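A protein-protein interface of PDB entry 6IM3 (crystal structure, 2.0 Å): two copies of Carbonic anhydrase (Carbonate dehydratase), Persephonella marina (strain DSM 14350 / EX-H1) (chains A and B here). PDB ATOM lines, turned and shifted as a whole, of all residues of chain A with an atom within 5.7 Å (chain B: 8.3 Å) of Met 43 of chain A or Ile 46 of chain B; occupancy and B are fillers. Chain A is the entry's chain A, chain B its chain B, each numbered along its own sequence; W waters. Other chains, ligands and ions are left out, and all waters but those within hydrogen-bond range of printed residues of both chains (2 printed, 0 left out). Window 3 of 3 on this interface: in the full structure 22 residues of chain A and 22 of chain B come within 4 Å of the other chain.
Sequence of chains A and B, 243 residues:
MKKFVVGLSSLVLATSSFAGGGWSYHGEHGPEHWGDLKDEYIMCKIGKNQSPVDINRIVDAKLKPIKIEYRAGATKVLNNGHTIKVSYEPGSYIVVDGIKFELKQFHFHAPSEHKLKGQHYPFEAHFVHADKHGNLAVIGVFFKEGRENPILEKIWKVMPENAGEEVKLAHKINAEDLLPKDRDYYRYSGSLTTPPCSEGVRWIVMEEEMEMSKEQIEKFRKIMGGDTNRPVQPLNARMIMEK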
ATOM      1  N   ASP A  39       0.841 -17.676  -6.363  1.00  0.00           N
ATOM      2  CA  ASP A  39       0.143 -16.953  -7.439  1.00  0.00           C
ATOM      3  C   ASP A  39       0.306 -17.645  -8.792  1.00  0.00           C
ATOM      4  O   ASP A  39      -0.646 -17.722  -9.549  1.00  0.00           O
ATOM      5  CB  ASP A  39       0.641 -15.504  -7.544  1.00  0.00           C
ATOM      6  CG  ASP A  39       0.111 -14.600  -6.398  1.00  0.00           C
ATOM      7  OD1 ASP A  39      -0.606 -15.074  -5.492  1.00  0.00           O
ATOM      8  OD2 ASP A  39       0.435 -13.392  -6.417  1.00  0.00           O
ATOM      9  N   GLU A  40       1.489 -18.188  -9.046  1.00  0.00           N
ATOM     10  CA  GLU A  40       1.788 -18.879 -10.322  1.00  0.00           C
ATOM     11  C   GLU A  40       0.949 -20.158 -10.527  1.00  0.00           C
ATOM     12  O   GLU A  40       0.899 -20.654 -11.621  1.00  0.00           O
ATOM     13  CB  GLU A  40       3.277 -19.242 -10.469  1.00  0.00           C
ATOM     14  CG  GLU A  40       4.242 -18.061 -10.317  1.00  0.00           C
ATOM     15  CD  GLU A  40       4.734 -17.888  -8.882  1.00  0.00           C
ATOM     16  OE1 GLU A  40       4.076 -17.152  -8.100  1.00  0.00           O
ATOM     17  OE2 GLU A  40       5.745 -18.539  -8.531  1.00  0.00           O
ATOM     18  N   TYR A  41       0.322 -20.664  -9.461  1.00  0.00           N
ATOM     19  CA  TYR A  41      -0.513 -21.879  -9.472  1.00  0.00           C
ATOM     20  C   TYR A  41      -1.988 -21.558  -9.542  1.00  0.00           C
ATOM     21  O   TYR A  41      -2.835 -22.416  -9.305  1.00  0.00           O
ATOM     22  CB  TYR A  41      -0.218 -22.735  -8.232  1.00  0.00           C
ATOM     23  CG  TYR A  41       1.216 -23.292  -8.107  1.00  0.00           C
ATOM     24  CD1 TYR A  41       2.189 -23.102  -9.091  1.00  0.00           C
ATOM     25  CD2 TYR A  41       1.564 -24.043  -7.003  1.00  0.00           C
ATOM     26  CE1 TYR A  41       3.497 -23.598  -8.948  1.00  0.00           C
ATOM     27  CE2 TYR A  41       2.861 -24.552  -6.850  1.00  0.00           C
ATOM     28  CZ  TYR A  41       3.814 -24.313  -7.807  1.00  0.00           C
ATOM     29  OH  TYR A  41       5.051 -24.887  -7.654  1.00  0.00           O
ATOM     30  N   ILE A  42      -2.311 -20.338  -9.968  1.00  0.00           N
ATOM     31  CA  ILE A  42      -3.700 -19.940 -10.063  1.00  0.00           C
ATOM     32  C   ILE A  42      -4.611 -20.874 -10.918  1.00  0.00           C
ATOM     33  O   ILE A  42      -5.780 -21.096 -10.561  1.00  0.00           O
ATOM     34  CB  ILE A  42      -3.809 -18.457 -10.552  1.00  0.00           C
ATOM     35  CG1 ILE A  42      -5.245 -17.954 -10.348  1.00  0.00           C
ATOM     36  CG2 ILE A  42      -3.273 -18.271 -11.959  1.00  0.00           C
ATOM     37  CD1 ILE A  42      -5.386 -16.445 -10.432  1.00  0.00           C
ATOM     38  N   MET A  43      -4.087 -21.406 -12.033  1.00  0.00           N
ATOM     39  CA  MET A  43      -4.902 -22.345 -12.893  1.00  0.00           C
ATOM     40  C   MET A  43      -5.421 -23.565 -12.113  1.00  0.00           C
ATOM     41  O   MET A  43      -6.538 -24.028 -12.381  1.00  0.00           O
ATOM     42  CB  MET A  43      -4.155 -22.759 -14.157  1.00  0.00           C
ATOM     43  CG  MET A  43      -4.063 -21.674 -15.222  1.00  0.00           C
ATOM     44  SD  MET A  43      -5.582 -20.842 -15.746  1.00  0.00           S
ATOM     45  CE  MET A  43      -6.519 -22.200 -16.106  1.00  0.00           C
ATOM     46  N   CYS A  44      -4.623 -24.052 -11.143  1.00  0.00           N
ATOM     47  CA  CYS A  44      -4.968 -25.233 -10.327  1.00  0.00           C
ATOM     48  C   CYS A  44      -6.279 -24.941  -9.557  1.00  0.00           C
ATOM     49  O   CYS A  44      -7.060 -25.820  -9.324  1.00  0.00           O
ATOM     50  CB  CYS A  44      -3.760 -25.761  -9.428  1.00  0.00           C
ATOM     51  SG  CYS A  44      -2.131 -26.235 -10.213  1.00  0.00           S
ATOM     52  N   LYS A  45      -6.574 -23.665  -9.362  1.00  0.00           N
ATOM     53  CA  LYS A  45      -7.778 -23.181  -8.709  1.00  0.00           C
ATOM     54  C   LYS A  45      -8.907 -22.667  -9.583  1.00  0.00           C
ATOM     55  O   LYS A  45     -10.061 -22.952  -9.306  1.00  0.00           O
ATOM     56  CB  LYS A  45      -7.395 -21.990  -7.806  1.00  0.00           C
ATOM     57  CG  LYS A  45      -8.474 -21.572  -6.816  1.00  0.00           C
ATOM     58  CD  LYS A  45      -7.996 -20.505  -5.840  1.00  0.00           C
ATOM     59  CE  LYS A  45      -8.844 -20.572  -4.576  1.00  0.00           C
ATOM     60  NZ  LYS A  45      -8.323 -19.686  -3.510  1.00  0.00           N
ATOM     61  N   ILE A  46      -8.607 -21.859 -10.596  1.00  0.00           N
ATOM     62  CA  ILE A  46      -9.701 -21.262 -11.430  1.00  0.00           C
ATOM     63  C   ILE A  46      -9.906 -21.932 -12.785  1.00  0.00           C
ATOM     64  O   ILE A  46     -10.868 -21.659 -13.487  1.00  0.00           O
ATOM     65  CB  ILE A  46      -9.491 -19.756 -11.656  1.00  0.00           C
ATOM     66  CG1 ILE A  46      -8.184 -19.478 -12.396  1.00  0.00           C
ATOM     67  CG2 ILE A  46      -9.478 -19.037 -10.303  1.00  0.00           C
ATOM     68  CD1 ILE A  46      -8.144 -18.106 -13.011  1.00  0.00           C
ATOM     69  N   GLY A  47      -8.989 -22.820 -13.160  1.00  0.00           N
ATOM     70  CA  GLY A  47      -9.044 -23.471 -14.485  1.00  0.00           C
ATOM     71  C   GLY A  47     -10.265 -24.320 -14.674  1.00  0.00           C
ATOM     72  O   GLY A  47     -10.721 -24.988 -13.768  1.00  0.00           O
ATOM     73  N   LYS A  48     -10.840 -24.222 -15.850  1.00  0.00           N
ATOM     74  CA  LYS A  48     -11.973 -25.037 -16.251  1.00  0.00           C
ATOM     75  C   LYS A  48     -11.670 -26.138 -17.288  1.00  0.00           C
ATOM     76  O   LYS A  48     -12.595 -26.815 -17.763  1.00  0.00           O
ATOM     77  CB  LYS A  48     -13.072 -24.129 -16.800  1.00  0.00           C
ATOM     78  CG  LYS A  48     -13.557 -23.045 -15.818  1.00  0.00           C
ATOM     79  CD  LYS A  48     -14.435 -23.694 -14.762  1.00  0.00           C
ATOM     80  CE  LYS A  48     -15.077 -22.629 -13.884  1.00  0.00           C
ATOM     81  NZ  LYS A  48     -16.256 -23.211 -13.197  1.00  0.00           N
ATOM     82  N   GLN A  50      -8.887 -28.475 -16.937  1.00  0.00           N
ATOM     83  CA  GLN A  50      -7.857 -29.182 -16.214  1.00  0.00           C
ATOM     84  C   GLN A  50      -7.859 -30.678 -16.468  1.00  0.00           C
ATOM     85  O   GLN A  50      -8.831 -31.258 -16.934  1.00  0.00           O
ATOM     86  CB  GLN A  50      -7.980 -28.926 -14.683  1.00  0.00           C
ATOM     87  CG  GLN A  50      -7.793 -27.469 -14.257  1.00  0.00           C
ATOM     88  CD  GLN A  50      -6.348 -27.101 -14.221  1.00  0.00           C
ATOM     89  OE1 GLN A  50      -5.598 -27.577 -13.348  1.00  0.00           O
ATOM     90  NE2 GLN A  50      -5.899 -26.353 -15.210  1.00  0.00           N
ATOM     91  N   PRO A 196       2.516 -25.739 -12.368  1.00  0.00           N
ATOM     92  CA  PRO A 196       1.400 -24.779 -12.353  1.00  0.00           C
ATOM     93  C   PRO A 196       0.114 -25.185 -13.068  1.00  0.00           C
ATOM     94  O   PRO A 196      -0.802 -24.365 -13.155  1.00  0.00           O
ATOM     95  CB  PRO A 196       2.020 -23.539 -13.029  1.00  0.00           C
ATOM     96  CG  PRO A 196       3.072 -24.055 -13.968  1.00  0.00           C
ATOM     97  CD  PRO A 196       3.567 -25.381 -13.370  1.00  0.00           C
ATOM     98  N   CYS A 197       0.013 -26.431 -13.525  1.00  0.00           N
ATOM     99  CA  CYS A 197      -1.239 -26.921 -14.165  1.00  0.00           C
ATOM    100  C   CYS A 197      -1.696 -26.060 -15.348  1.00  0.00           C
ATOM    101  O   CYS A 197      -2.870 -25.732 -15.493  1.00  0.00           O
ATOM    102  CB  CYS A 197      -2.351 -27.022 -13.161  1.00  0.00           C
ATOM    103  SG  CYS A 197      -2.064 -28.050 -11.685  1.00  0.00           S
ATOM    104  N   SER A 198      -0.716 -25.675 -16.154  1.00  0.00           N
ATOM    105  CA  SER A 198      -0.903 -24.812 -17.315  1.00  0.00           C
ATOM    106  C   SER A 198      -1.829 -25.474 -18.309  1.00  0.00           C
ATOM    107  O   SER A 198      -1.732 -26.695 -18.562  1.00  0.00           O
ATOM    108  CB  SER A 198       0.467 -24.596 -18.038  1.00  0.00           C
ATOM    109  OG  SER A 198       1.398 -24.212 -17.067  1.00  0.00           O
ATOM    110  N   GLU A 199      -2.720 -24.674 -18.880  1.00  0.00           N
ATOM    111  CA  GLU A 199      -3.709 -25.122 -19.859  1.00  0.00           C
ATOM    112  C   GLU A 199      -3.193 -24.966 -21.305  1.00  0.00           C
ATOM    113  O   GLU A 199      -2.033 -24.658 -21.508  1.00  0.00           O
ATOM    114  CB  GLU A 199      -5.079 -24.459 -19.607  1.00  0.00           C
ATOM    115  CG  GLU A 199      -5.710 -25.062 -18.340  1.00  0.00           C
ATOM    116  CD  GLU A 199      -7.105 -24.569 -18.054  1.00  0.00           C
ATOM    117  OE1 GLU A 199      -7.677 -23.773 -18.854  1.00  0.00           O
ATOM    118  OE2 GLU A 199      -7.729 -25.039 -17.047  1.00  0.00           O
ATOM    119  N   ARG A 230      -2.956 -37.035  -9.438  1.00  0.00           N
ATOM    120  CA  ARG A 230      -3.788 -35.903  -9.149  1.00  0.00           C
ATOM    121  C   ARG A 230      -5.218 -36.382  -9.305  1.00  0.00           C
ATOM    122  O   ARG A 230      -5.501 -37.117 -10.211  1.00  0.00           O
ATOM    123  CB  ARG A 230      -3.555 -34.777 -10.140  1.00  0.00           C
ATOM    124  CG  ARG A 230      -4.440 -33.595  -9.900  1.00  0.00           C
ATOM    125  CD  ARG A 230      -4.329 -32.534 -10.968  1.00  0.00           C
ATOM    126  NE  ARG A 230      -4.994 -31.328 -10.544  1.00  0.00           N
ATOM    127  CZ  ARG A 230      -5.182 -30.270 -11.289  1.00  0.00           C
ATOM    128  NH1 ARG A 230      -4.768 -30.242 -12.515  1.00  0.00           N
ATOM    129  NH2 ARG A 230      -5.768 -29.232 -10.783  1.00  0.00           N
ATOM    130  N   GLY B  35      -7.018  -7.586 -20.323  1.00  0.00           N
ATOM    131  CA  GLY B  35      -6.418  -8.416 -19.253  1.00  0.00           C
ATOM    132  C   GLY B  35      -5.599  -7.647 -18.224  1.00  0.00           C
ATOM    133  O   GLY B  35      -5.461  -8.085 -17.072  1.00  0.00           O
ATOM    134  N   ASP B  39      -7.646  -7.308 -12.032  1.00  0.00           N
ATOM    135  CA  ASP B  39      -7.319  -8.669 -11.614  1.00  0.00           C
ATOM    136  C   ASP B  39      -8.397  -9.681 -12.027  1.00  0.00           C
ATOM    137  O   ASP B  39      -8.070 -10.778 -12.443  1.00  0.00           O
ATOM    138  CB  ASP B  39      -7.099  -8.737 -10.084  1.00  0.00           C
ATOM    139  CG  ASP B  39      -5.772  -8.102  -9.643  1.00  0.00           C
ATOM    140  OD1 ASP B  39      -5.020  -7.555 -10.483  1.00  0.00           O
ATOM    141  OD2 ASP B  39      -5.479  -8.150  -8.430  1.00  0.00           O
ATOM    142  N   TYR B  41     -10.103  -9.859 -14.602  1.00  0.00           N
ATOM    143  CA  TYR B  41     -10.045 -10.077 -16.055  1.00  0.00           C
ATOM    144  C   TYR B  41      -8.802 -10.857 -16.458  1.00  0.00           C
ATOM    145  O   TYR B  41      -8.416 -10.889 -17.620  1.00  0.00           O
ATOM    146  CB  TYR B  41     -10.068  -8.737 -16.780  1.00  0.00           C
ATOM    147  CG  TYR B  41     -11.324  -7.895 -16.608  1.00  0.00           C
ATOM    148  CD1 TYR B  41     -12.438  -8.333 -15.880  1.00  0.00           C
ATOM    149  CD2 TYR B  41     -11.407  -6.631 -17.215  1.00  0.00           C
ATOM    150  CE1 TYR B  41     -13.602  -7.552 -15.758  1.00  0.00           C
ATOM    151  CE2 TYR B  41     -12.561  -5.845 -17.083  1.00  0.00           C
ATOM    152  CZ  TYR B  41     -13.643  -6.303 -16.359  1.00  0.00           C
ATOM    153  OH  TYR B  41     -14.788  -5.539 -16.284  1.00  0.00           O
ATOM    154  N   ILE B  42      -8.195 -11.547 -15.508  1.00  0.00           N
ATOM    155  CA  ILE B  42      -6.988 -12.333 -15.761  1.00  0.00           C
ATOM    156  C   ILE B  42      -7.112 -13.379 -16.898  1.00  0.00           C
ATOM    157  O   ILE B  42      -6.167 -13.533 -17.691  1.00  0.00           O
ATOM    158  CB  ILE B  42      -6.465 -13.002 -14.447  1.00  0.00           C
ATOM    159  CG1 ILE B  42      -5.049 -13.546 -14.682  1.00  0.00           C
ATOM    160  CG2 ILE B  42      -7.450 -14.033 -13.900  1.00  0.00           C
ATOM    161  CD1 ILE B  42      -4.307 -13.894 -13.415  1.00  0.00           C
ATOM    162  N   MET B  43      -8.277 -14.023 -17.030  1.00  0.00           N
ATOM    163  CA  MET B  43      -8.491 -15.010 -18.154  1.00  0.00           C
ATOM    164  C   MET B  43      -8.291 -14.399 -19.529  1.00  0.00           C
ATOM    165  O   MET B  43      -7.775 -15.064 -20.438  1.00  0.00           O
ATOM    166  CB  MET B  43      -9.847 -15.700 -18.053  1.00  0.00           C
ATOM    167  CG  MET B  43      -9.928 -16.776 -16.959  1.00  0.00           C
ATOM    168  SD  MET B  43      -8.625 -18.058 -16.899  1.00  0.00           S
ATOM    169  CE  MET B  43      -8.679 -18.592 -18.486  1.00  0.00           C
ATOM    170  N   CYS B  44      -8.674 -13.113 -19.678  1.00  0.00           N
ATOM    171  CA  CYS B  44      -8.563 -12.377 -20.944  1.00  0.00           C
ATOM    172  C   CYS B  44      -7.073 -12.350 -21.361  1.00  0.00           C
ATOM    173  O   CYS B  44      -6.755 -12.357 -22.554  1.00  0.00           O
ATOM    174  CB  CYS B  44      -9.307 -10.961 -20.953  1.00  0.00           C
ATOM    175  SG  CYS B  44     -11.111 -10.829 -20.553  1.00  0.00           S
ATOM    176  N   LYS B  45      -6.186 -12.499 -20.392  1.00  0.00           N
ATOM    177  CA  LYS B  45      -4.737 -12.522 -20.606  1.00  0.00           C
ATOM    178  C   LYS B  45      -4.050 -13.894 -20.615  1.00  0.00           C
ATOM    179  O   LYS B  45      -3.167 -14.119 -21.426  1.00  0.00           O
ATOM    180  CB  LYS B  45      -4.061 -11.717 -19.481  1.00  0.00           C
ATOM    181  CG  LYS B  45      -2.594 -11.394 -19.721  1.00  0.00           C
ATOM    182  CD  LYS B  45      -2.026 -10.458 -18.662  1.00  0.00           C
ATOM    183  CE  LYS B  45      -0.824  -9.719 -19.239  1.00  0.00           C
ATOM    184  NZ  LYS B  45      -0.336  -8.655 -18.336  1.00  0.00           N
ATOM    185  N   ILE B  46      -4.377 -14.764 -19.676  1.00  0.00           N
ATOM    186  CA  ILE B  46      -3.674 -16.050 -19.573  1.00  0.00           C
ATOM    187  C   ILE B  46      -4.479 -17.264 -20.136  1.00  0.00           C
ATOM    188  O   ILE B  46      -3.943 -18.353 -20.249  1.00  0.00           O
ATOM    189  CB  ILE B  46      -3.246 -16.371 -18.125  1.00  0.00           C
ATOM    190  CG1 ILE B  46      -4.461 -16.486 -17.207  1.00  0.00           C
ATOM    191  CG2 ILE B  46      -2.312 -15.301 -17.614  1.00  0.00           C
ATOM    192  CD1 ILE B  46      -4.156 -17.194 -15.911  1.00  0.00           C
ATOM    193  N   GLY B  47      -5.739 -17.074 -20.409  1.00  0.00           N
ATOM    194  CA  GLY B  47      -6.616 -18.143 -20.890  1.00  0.00           C
ATOM    195  C   GLY B  47      -6.140 -18.751 -22.180  1.00  0.00           C
ATOM    196  O   GLY B  47      -5.674 -18.041 -23.089  1.00  0.00           O
ATOM    197  N   LYS B  48      -6.173 -20.074 -22.249  1.00  0.00           N
ATOM    198  CA  LYS B  48      -5.856 -20.832 -23.475  1.00  0.00           C
ATOM    199  C   LYS B  48      -7.067 -21.458 -24.173  1.00  0.00           C
ATOM    200  O   LYS B  48      -6.922 -22.132 -25.197  1.00  0.00           O
ATOM    201  CB  LYS B  48      -4.870 -21.911 -23.122  1.00  0.00           C
ATOM    202  CG  LYS B  48      -3.559 -21.410 -22.497  1.00  0.00           C
ATOM    203  CD  LYS B  48      -2.705 -20.749 -23.582  1.00  0.00           C
ATOM    204  CE  LYS B  48      -1.339 -20.387 -23.036  1.00  0.00           C
ATOM    205  NZ  LYS B  48      -0.406 -20.217 -24.153  1.00  0.00           N
ATOM    206  N   ASN B  49      -8.262 -21.191 -23.661  1.00  0.00           N
ATOM    207  CA  ASN B  49      -9.534 -21.656 -24.178  1.00  0.00           C
ATOM    208  C   ASN B  49     -10.568 -20.550 -24.329  1.00  0.00           C
ATOM    209  O   ASN B  49     -11.707 -20.637 -23.879  1.00  0.00           O
ATOM    210  CB  ASN B  49     -10.076 -22.788 -23.292  1.00  0.00           C
ATOM    211  CG  ASN B  49      -9.133 -24.004 -23.281  1.00  0.00           C
ATOM    212  OD1 ASN B  49      -9.184 -24.834 -24.176  1.00  0.00           O
ATOM    213  ND2 ASN B  49      -8.244 -24.074 -22.325  1.00  0.00           N
ATOM    214  N   GLN B  50     -10.123 -19.500 -25.006  1.00  0.00           N
ATOM    215  CA  GLN B  50     -10.921 -18.276 -25.217  1.00  0.00           C
ATOM    216  C   GLN B  50     -11.682 -18.268 -26.493  1.00  0.00           C
ATOM    217  O   GLN B  50     -11.411 -19.067 -27.433  1.00  0.00           O
ATOM    218  CB  GLN B  50      -9.987 -17.035 -25.211  1.00  0.00           C
ATOM    219  CG  GLN B  50      -9.234 -16.799 -23.898  1.00  0.00           C
ATOM    220  CD  GLN B  50     -10.169 -16.156 -22.890  1.00  0.00           C
ATOM    221  OE1 GLN B  50     -10.534 -14.969 -23.046  1.00  0.00           O
ATOM    222  NE2 GLN B  50     -10.597 -16.923 -21.884  1.00  0.00           N
ATOM    223  N   GLU B 199     -13.979 -18.968 -18.637  1.00  0.00           N
ATOM    224  CA  GLU B 199     -13.890 -20.210 -19.389  1.00  0.00           C
ATOM    225  C   GLU B 199     -14.906 -21.249 -18.882  1.00  0.00           C
ATOM    226  O   GLU B 199     -15.740 -20.960 -18.033  1.00  0.00           O
ATOM    227  CB  GLU B 199     -12.425 -20.684 -19.443  1.00  0.00           C
ATOM    228  CG  GLU B 199     -11.640 -19.811 -20.408  1.00  0.00           C
ATOM    229  CD  GLU B 199     -10.209 -20.253 -20.645  1.00  0.00           C
ATOM    230  OE1 GLU B 199      -9.793 -21.311 -20.109  1.00  0.00           O
ATOM    231  OE2 GLU B 199      -9.488 -19.566 -21.438  1.00  0.00           O
ATOM    232  N   ARG B 230     -15.061  -9.022 -30.426  1.00  0.00           N
ATOM    233  CA  ARG B 230     -13.733  -9.315 -29.935  1.00  0.00           C
ATOM    234  C   ARG B 230     -12.926  -9.995 -31.047  1.00  0.00           C
ATOM    235  O   ARG B 230     -13.475 -10.870 -31.731  1.00  0.00           O
ATOM    236  CB  ARG B 230     -13.827 -10.217 -28.691  1.00  0.00           C
ATOM    237  CG  ARG B 230     -12.471 -10.567 -28.125  1.00  0.00           C
ATOM    238  CD  ARG B 230     -12.571 -11.585 -27.002  1.00  0.00           C
ATOM    239  NE  ARG B 230     -11.344 -11.663 -26.255  1.00  0.00           N
ATOM    240  CZ  ARG B 230     -11.079 -12.579 -25.320  1.00  0.00           C
ATOM    241  NH1 ARG B 230     -11.932 -13.584 -25.031  1.00  0.00           N
ATOM    242  NH2 ARG B 230      -9.930 -12.487 -24.658  1.00  0.00           N
ATOM    243  N   ASN B 236      -5.306 -23.156 -29.918  1.00  0.00           N
ATOM    244  CA  ASN B 236      -4.386 -23.839 -29.049  1.00  0.00           C
ATOM    245  C   ASN B 236      -4.561 -25.350 -29.149  1.00  0.00           C
ATOM    246  O   ASN B 236      -4.403 -25.881 -30.201  1.00  0.00           O
ATOM    247  CB  ASN B 236      -4.477 -23.266 -27.647  1.00  0.00           C
ATOM    248  CG  ASN B 236      -3.912 -21.859 -27.552  1.00  0.00           C
ATOM    249  OD1 ASN B 236      -2.916 -21.539 -28.149  1.00  0.00           O
ATOM    250  ND2 ASN B 236      -4.545 -21.038 -26.791  1.00  0.00           N
HETATM  251  O   HOH W   1      -7.371 -21.666 -20.426  1.00  0.00           O
HETATM  252  O   HOH W   2      -9.835 -22.778 -18.114  1.00  0.00           O
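Met 43 of chain A touches Ile 46 of chain B, and with the chains exchanged Ile 46 of chain A touches Met 43 of chain B. Lys 48 of chain A touches Glu 199 of chain B, and with the chains exchanged Glu 199 of chain A touches Lys 48 of chain B. Glu 199 of chain B touches its own counterpart, Glu 199 of chain A. Of the 6 pairs that touch across the chains among the printed residues, 5 have their exchanged pair printed and touching as well.
OE1 of Glu 199 of chain A sits close to OE1 of Glu 199 of chain B (3.5 Å).
Of the 16 printed residues of chain A, 4 touch a printed residue of chain B. Hydrophobic or aromatic side chains of chain A that line the printed part of chain B: Met 43 and Ile 46. Along chain B the printed residues that touch a printed residue of chain A span positions 43 to 199. Among the printed residues, 6 pairs touch across the chains.
Ile 46 of chain B touches Met 43 of chain A (CD1 to SD, 3.9 Å). Met 43 of chain B touches Ile 46 of chain A. Lys 48 of chain A touches Glu 199 of chain B (CG to O, 3.7 Å). Glu 199 of chain A touches Lys 48 of chain B. Glu 199 of chain A touches Asn 49 of chain B (OE1 to ND2, 3.5 Å).
Water W1 lies within hydrogen-bond range of OE1 of Glu 199 of chain B (2.5 Å), OE1 of Glu 199 of chain A (2.6 Å), N of Lys 48 of chain B (2.7 Å) and ND2 of Asn 49 of chain B (3.2 Å). Water W2 lies within hydrogen-bond range of OE1 of Glu 199 of chain B (2.5 Å), OE1 of Glu 199 of chain A (2.5 Å) and N of Lys 48 of chain A (2.9 Å).
The side-chain carboxylate (OE2) of Glu 199 of chain B is in hydrogen-bond range of the backbone NH (N) of Asn 49 of chain B (3.0 Å). The side-chain amide nitrogen of Gln 50 of chain B sits at hydrogen-bond distance from the side-chain carboxylate of Glu 199 of chain B, 2.9 Å away. The backbone NH of Lys 48 of chain B sits at hydrogen-bond distance from the side-chain carboxylate of Glu 199 of chain B (3.5 Å). The backbone carbonyl oxygen of Lys 48 of chain B lies within hydrogen-bond range of the side-chain amide nitrogen of Asn 236 of chain B. The backbone NH (N) of Lys 48 of chain A sits at hydrogen-bond distance from the side-chain carboxylate (OE2) of Glu 199 of chain A (3.4 Å). The side-chain sulfur (SG) of Cys 44 of chain A is disulfide-bonded to the side-chain sulfur (SG) of Cys 197 of chain A (2.3 Å).
Printed residues of chain B within 4 Å of Met 43 of chain A: Ile 46. Printed residues of chain B within 4 Å of Ile 46 of chain A: Met 43 (3.9 Å). Of the printed residues of chain B, Lys 48 of chain A touches Glu 199 (3.7 Å). Cys 197 of chain A touches none of the printed residues of chain B. Of the printed residues of chain A, Ile 46 of chain B touches Met 43. Printed residues of chain A within 4 Å of Glu 199 of chain B: Lys 48 and Glu 199. Arg 230 of chain B touches none of the printed residues of chain A. The nearest residue of chain B that does not touch Met 43 of chain A is Met 43 of chain B (4.3 Å).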
